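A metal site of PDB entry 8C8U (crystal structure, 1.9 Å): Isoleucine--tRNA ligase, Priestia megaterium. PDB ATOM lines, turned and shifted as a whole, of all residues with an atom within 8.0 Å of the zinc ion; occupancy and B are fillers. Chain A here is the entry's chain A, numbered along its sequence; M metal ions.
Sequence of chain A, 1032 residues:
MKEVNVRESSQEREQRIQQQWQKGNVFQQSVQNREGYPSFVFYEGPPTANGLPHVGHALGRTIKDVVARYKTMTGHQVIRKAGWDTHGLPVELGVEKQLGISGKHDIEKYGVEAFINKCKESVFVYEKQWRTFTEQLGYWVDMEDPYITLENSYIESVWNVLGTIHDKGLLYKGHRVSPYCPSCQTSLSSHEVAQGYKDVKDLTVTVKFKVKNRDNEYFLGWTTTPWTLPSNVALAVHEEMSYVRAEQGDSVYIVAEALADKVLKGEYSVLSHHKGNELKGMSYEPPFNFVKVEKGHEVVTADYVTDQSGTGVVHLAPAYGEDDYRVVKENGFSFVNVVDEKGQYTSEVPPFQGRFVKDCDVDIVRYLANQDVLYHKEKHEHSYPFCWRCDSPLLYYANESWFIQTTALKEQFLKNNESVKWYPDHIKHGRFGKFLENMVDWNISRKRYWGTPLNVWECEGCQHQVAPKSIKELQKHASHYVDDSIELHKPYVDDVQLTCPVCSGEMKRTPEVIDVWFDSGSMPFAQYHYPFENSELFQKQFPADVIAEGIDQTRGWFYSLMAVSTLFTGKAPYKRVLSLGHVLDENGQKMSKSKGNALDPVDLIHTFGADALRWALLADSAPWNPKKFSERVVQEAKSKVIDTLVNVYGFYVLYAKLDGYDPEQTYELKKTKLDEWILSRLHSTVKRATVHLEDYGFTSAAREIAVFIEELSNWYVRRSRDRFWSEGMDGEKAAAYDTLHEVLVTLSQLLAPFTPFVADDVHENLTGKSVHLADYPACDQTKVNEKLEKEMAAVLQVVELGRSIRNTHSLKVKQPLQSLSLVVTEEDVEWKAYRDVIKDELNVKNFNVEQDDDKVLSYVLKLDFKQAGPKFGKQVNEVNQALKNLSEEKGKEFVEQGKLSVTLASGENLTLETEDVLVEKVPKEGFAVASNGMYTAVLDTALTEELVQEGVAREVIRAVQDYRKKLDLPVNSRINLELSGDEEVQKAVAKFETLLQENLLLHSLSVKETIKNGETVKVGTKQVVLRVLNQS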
ATOM      1  N   TYR A 180       1.513  10.785  23.670  1.00  0.00           N
ATOM      2  CA  TYR A 180       0.084  11.048  23.785  1.00  0.00           C
ATOM      3  C   TYR A 180      -0.196  11.720  25.112  1.00  0.00           C
ATOM      4  O   TYR A 180       0.330  11.286  26.143  1.00  0.00           O
ATOM      5  CB  TYR A 180      -0.712   9.745  23.652  1.00  0.00           C
ATOM      6  CG  TYR A 180      -2.205   9.885  23.760  1.00  0.00           C
ATOM      7  CD1 TYR A 180      -2.973  10.270  22.656  1.00  0.00           C
ATOM      8  CD2 TYR A 180      -2.865   9.637  24.959  1.00  0.00           C
ATOM      9  CE1 TYR A 180      -4.345  10.409  22.740  1.00  0.00           C
ATOM     10  CE2 TYR A 180      -4.264   9.777  25.055  1.00  0.00           C
ATOM     11  CZ  TYR A 180      -4.988  10.164  23.935  1.00  0.00           C
ATOM     12  OH  TYR A 180      -6.365  10.292  23.993  1.00  0.00           O
ATOM     13  N   CYS A 181      -1.011  12.779  25.103  1.00  0.00           N
ATOM     14  CA  CYS A 181      -1.443  13.355  26.367  1.00  0.00           C
ATOM     15  C   CYS A 181      -2.821  12.829  26.704  1.00  0.00           C
ATOM     16  O   CYS A 181      -3.746  12.985  25.894  1.00  0.00           O
ATOM     17  CB  CYS A 181      -1.481  14.873  26.329  1.00  0.00           C
ATOM     18  SG  CYS A 181      -2.110  15.472  27.910  1.00  0.00           S
ATOM     19  N   PRO A 182      -3.004  12.187  27.866  1.00  0.00           N
ATOM     20  CA  PRO A 182      -4.335  11.657  28.218  1.00  0.00           C
ATOM     21  C   PRO A 182      -5.307  12.722  28.687  1.00  0.00           C
ATOM     22  O   PRO A 182      -6.514  12.437  28.793  1.00  0.00           O
ATOM     23  CB  PRO A 182      -4.018  10.669  29.351  1.00  0.00           C
ATOM     24  CG  PRO A 182      -2.748  11.193  29.951  1.00  0.00           C
ATOM     25  CD  PRO A 182      -1.964  11.739  28.809  1.00  0.00           C
ATOM     26  N   SER A 183      -4.812  13.931  28.987  1.00  0.00           N
ATOM     27  CA  SER A 183      -5.664  15.036  29.408  1.00  0.00           C
ATOM     28  C   SER A 183      -6.225  15.787  28.202  1.00  0.00           C
ATOM     29  O   SER A 183      -7.440  15.880  28.025  1.00  0.00           O
ATOM     30  CB  SER A 183      -4.857  15.984  30.316  1.00  0.00           C
ATOM     31  OG  SER A 183      -5.687  16.934  30.958  1.00  0.00           O
ATOM     32  N   CYS A 184      -5.338  16.300  27.347  1.00  0.00           N
ATOM     33  CA  CYS A 184      -5.773  16.964  26.120  1.00  0.00           C
ATOM     34  C   CYS A 184      -6.331  15.977  25.093  1.00  0.00           C
ATOM     35  O   CYS A 184      -7.003  16.410  24.153  1.00  0.00           O
ATOM     36  CB  CYS A 184      -4.613  17.738  25.463  1.00  0.00           C
ATOM     37  SG  CYS A 184      -3.570  18.718  26.568  1.00  0.00           S
ATOM     38  N   GLN A 185      -6.054  14.680  25.242  1.00  0.00           N
ATOM     39  CA  GLN A 185      -6.438  13.646  24.285  1.00  0.00           C
ATOM     40  C   GLN A 185      -5.915  13.979  22.886  1.00  0.00           C
ATOM     41  O   GLN A 185      -6.669  14.094  21.919  1.00  0.00           O
ATOM     42  CB  GLN A 185      -7.954  13.443  24.272  1.00  0.00           C
ATOM     43  CG  GLN A 185      -8.560  13.132  25.648  1.00  0.00           C
ATOM     44  CD  GLN A 185     -10.051  12.795  25.591  1.00  0.00           C
ATOM     45  OE1 GLN A 185     -10.548  12.301  24.570  1.00  0.00           O
ATOM     46  NE2 GLN A 185     -10.755  13.053  26.688  1.00  0.00           N
ATOM     47  N   THR A 186      -4.585  14.099  22.784  1.00  0.00           N
ATOM     48  CA  THR A 186      -3.940  14.411  21.508  1.00  0.00           C
ATOM     49  C   THR A 186      -2.501  13.896  21.500  1.00  0.00           C
ATOM     50  O   THR A 186      -1.850  13.783  22.540  1.00  0.00           O
ATOM     51  CB  THR A 186      -3.935  15.923  21.224  1.00  0.00           C
ATOM     52  OG1 THR A 186      -3.104  16.198  20.089  1.00  0.00           O
ATOM     53  CG2 THR A 186      -3.399  16.691  22.398  1.00  0.00           C
ATOM     54  N   LEU A 188       1.402  14.340  20.642  1.00  0.00           N
ATOM     55  CA  LEU A 188       2.381  15.414  20.621  1.00  0.00           C
ATOM     56  C   LEU A 188       3.547  15.062  19.703  1.00  0.00           C
ATOM     57  O   LEU A 188       3.854  13.891  19.470  1.00  0.00           O
ATOM     58  CB  LEU A 188       2.901  15.706  22.036  1.00  0.00           C
ATOM     59  CG  LEU A 188       1.934  16.280  23.073  1.00  0.00           C
ATOM     60  CD1 LEU A 188       0.954  15.226  23.575  1.00  0.00           C
ATOM     61  CD2 LEU A 188       2.679  16.890  24.238  1.00  0.00           C
ATOM     62  N   PHE A 386       6.445  15.340  30.021  1.00  0.00           N
ATOM     63  CA  PHE A 386       5.133  15.820  30.421  1.00  0.00           C
ATOM     64  C   PHE A 386       4.551  16.692  29.333  1.00  0.00           C
ATOM     65  O   PHE A 386       5.231  17.100  28.383  1.00  0.00           O
ATOM     66  CB  PHE A 386       5.195  16.598  31.738  1.00  0.00           C
ATOM     67  CG  PHE A 386       5.335  15.723  32.946  1.00  0.00           C
ATOM     68  CD1 PHE A 386       6.562  15.155  33.265  1.00  0.00           C
ATOM     69  CD2 PHE A 386       4.261  15.501  33.782  1.00  0.00           C
ATOM     70  CE1 PHE A 386       6.706  14.363  34.384  1.00  0.00           C
ATOM     71  CE2 PHE A 386       4.389  14.705  34.906  1.00  0.00           C
ATOM     72  CZ  PHE A 386       5.616  14.134  35.203  1.00  0.00           C
ATOM     73  N   CYS A 387       3.263  17.004  29.485  1.00  0.00           N
ATOM     74  CA  CYS A 387       2.534  17.816  28.528  1.00  0.00           C
ATOM     75  C   CYS A 387       2.780  19.294  28.838  1.00  0.00           C
ATOM     76  O   CYS A 387       2.299  19.801  29.853  1.00  0.00           O
ATOM     77  CB  CYS A 387       1.052  17.477  28.570  1.00  0.00           C
ATOM     78  SG  CYS A 387       0.081  18.331  27.334  1.00  0.00           S
ATOM     79  N   TRP A 388       3.509  19.988  27.950  1.00  0.00           N
ATOM     80  CA  TRP A 388       3.704  21.428  28.115  1.00  0.00           C
ATOM     81  C   TRP A 388       2.375  22.143  28.369  1.00  0.00           C
ATOM     82  O   TRP A 388       2.343  23.132  29.109  1.00  0.00           O
ATOM     83  CB  TRP A 388       4.380  22.014  26.870  1.00  0.00           C
ATOM     84  CG  TRP A 388       3.500  22.010  25.627  1.00  0.00           C
ATOM     85  CD1 TRP A 388       3.462  21.055  24.655  1.00  0.00           C
ATOM     86  CD2 TRP A 388       2.542  23.010  25.252  1.00  0.00           C
ATOM     87  NE1 TRP A 388       2.540  21.392  23.694  1.00  0.00           N
ATOM     88  CE2 TRP A 388       1.960  22.585  24.035  1.00  0.00           C
ATOM     89  CE3 TRP A 388       2.115  24.219  25.811  1.00  0.00           C
ATOM     90  CZ2 TRP A 388       0.972  23.329  23.373  1.00  0.00           C
ATOM     91  CZ3 TRP A 388       1.142  24.950  25.151  1.00  0.00           C
ATOM     92  CH2 TRP A 388       0.580  24.504  23.946  1.00  0.00           C
ATOM     93  N   ARG A 389       1.285  21.631  27.791  1.00  0.00           N
ATOM     94  CA  ARG A 389      -0.002  22.298  27.832  1.00  0.00           C
ATOM     95  C   ARG A 389      -0.778  22.053  29.122  1.00  0.00           C
ATOM     96  O   ARG A 389      -1.670  22.843  29.445  1.00  0.00           O
ATOM     97  CB  ARG A 389      -0.843  21.850  26.628  1.00  0.00           C
ATOM     98  CG  ARG A 389      -1.924  22.839  26.220  1.00  0.00           C
ATOM     99  CD  ARG A 389      -2.483  22.536  24.832  1.00  0.00           C
ATOM    100  NE  ARG A 389      -2.800  23.767  24.113  1.00  0.00           N
ATOM    101  CZ  ARG A 389      -3.944  24.442  24.216  1.00  0.00           C
ATOM    102  NH1 ARG A 389      -4.910  24.015  25.020  1.00  0.00           N
ATOM    103  NH2 ARG A 389      -4.125  25.557  23.516  1.00  0.00           N
ATOM    104  N   CYS A 390      -0.474  20.967  29.870  1.00  0.00           N
ATOM    105  CA  CYS A 390      -1.125  20.775  31.161  1.00  0.00           C
ATOM    106  C   CYS A 390      -0.262  20.087  32.205  1.00  0.00           C
ATOM    107  O   CYS A 390      -0.753  19.836  33.310  1.00  0.00           O
ATOM    108  CB  CYS A 390      -2.444  19.983  30.981  1.00  0.00           C
ATOM    109  SG  CYS A 390      -2.262  18.242  30.452  1.00  0.00           S
ATOM    110  N   ASP A 391       1.017  19.821  31.919  1.00  0.00           N
ATOM    111  CA  ASP A 391       1.915  18.942  32.692  1.00  0.00           C
ATOM    112  C   ASP A 391       1.222  17.709  33.271  1.00  0.00           C
ATOM    113  O   ASP A 391       1.570  17.247  34.364  1.00  0.00           O
ATOM    114  CB  ASP A 391       2.659  19.724  33.788  1.00  0.00           C
ATOM    115  CG  ASP A 391       1.753  20.467  34.745  1.00  0.00           C
ATOM    116  OD1 ASP A 391       0.976  19.816  35.486  1.00  0.00           O
ATOM    117  OD2 ASP A 391       1.828  21.711  34.780  1.00  0.00           O
ATOM    118  N   SER A 392       0.276  17.138  32.533  1.00  0.00           N
ATOM    119  CA  SER A 392      -0.046  15.736  32.734  1.00  0.00           C
ATOM    120  C   SER A 392       1.105  14.888  32.205  1.00  0.00           C
ATOM    121  O   SER A 392       1.750  15.263  31.214  1.00  0.00           O
ATOM    122  CB  SER A 392      -1.351  15.355  32.038  1.00  0.00           C
ATOM    123  OG  SER A 392      -1.524  13.947  31.910  1.00  0.00           O
ATOM    124  N   PRO A 393       1.441  13.775  32.849  1.00  0.00           N
ATOM    125  CA  PRO A 393       2.429  12.866  32.260  1.00  0.00           C
ATOM    126  C   PRO A 393       1.951  12.382  30.891  1.00  0.00           C
ATOM    127  O   PRO A 393       0.748  12.216  30.669  1.00  0.00           O
ATOM    128  CB  PRO A 393       2.521  11.715  33.278  1.00  0.00           C
ATOM    129  CG  PRO A 393       1.216  11.785  34.050  1.00  0.00           C
ATOM    130  CD  PRO A 393       0.865  13.246  34.098  1.00  0.00           C
ATOM    131  N   LEU A 394       2.889  12.196  29.967  1.00  0.00           N
ATOM    132  CA  LEU A 394       2.541  11.644  28.669  1.00  0.00           C
ATOM    133  C   LEU A 394       2.521  10.106  28.726  1.00  0.00           C
ATOM    134  O   LEU A 394       2.881   9.488  29.732  1.00  0.00           O
ATOM    135  CB  LEU A 394       3.527  12.111  27.589  1.00  0.00           C
ATOM    136  CG  LEU A 394       3.632  13.584  27.200  1.00  0.00           C
ATOM    137  CD1 LEU A 394       4.589  13.722  26.034  1.00  0.00           C
ATOM    138  CD2 LEU A 394       2.271  14.175  26.852  1.00  0.00           C
HETATM  139 ZN    ZN M   1      -1.982  18.094  27.992  1.00  0.00          ZN
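N of Arg 389 sits close to SG of Cys 387 (3.5 Å).
The backbone NH of Cys 387 lies within hydrogen-bond range of the backbone carbonyl oxygen of Ser 392, 2.9 Å away.
The side-chain hydroxyl (OG) of Ser 183 lies close to the side-chain sulfur (SG) of Cys 390 (3.7 Å).
The backbone NH (N) of Ser 392 sits close to the side-chain sulfur (SG) of Cys 390 (3.5 Å).
N of Ser 183 sits close to SG of Cys 181 (3.3 Å).
The backbone NH (N) of Cys 181 is in hydrogen-bond range of the backbone carbonyl oxygen (O) of Thr 186 (2.9 Å).
The zinc ion is bound by SG of Cys 387 (2.2 Å), SG of Cys 184 (2.2 Å), SG of Cys 390 (2.5 Å) and SG of Cys 181 (2.6 Å).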
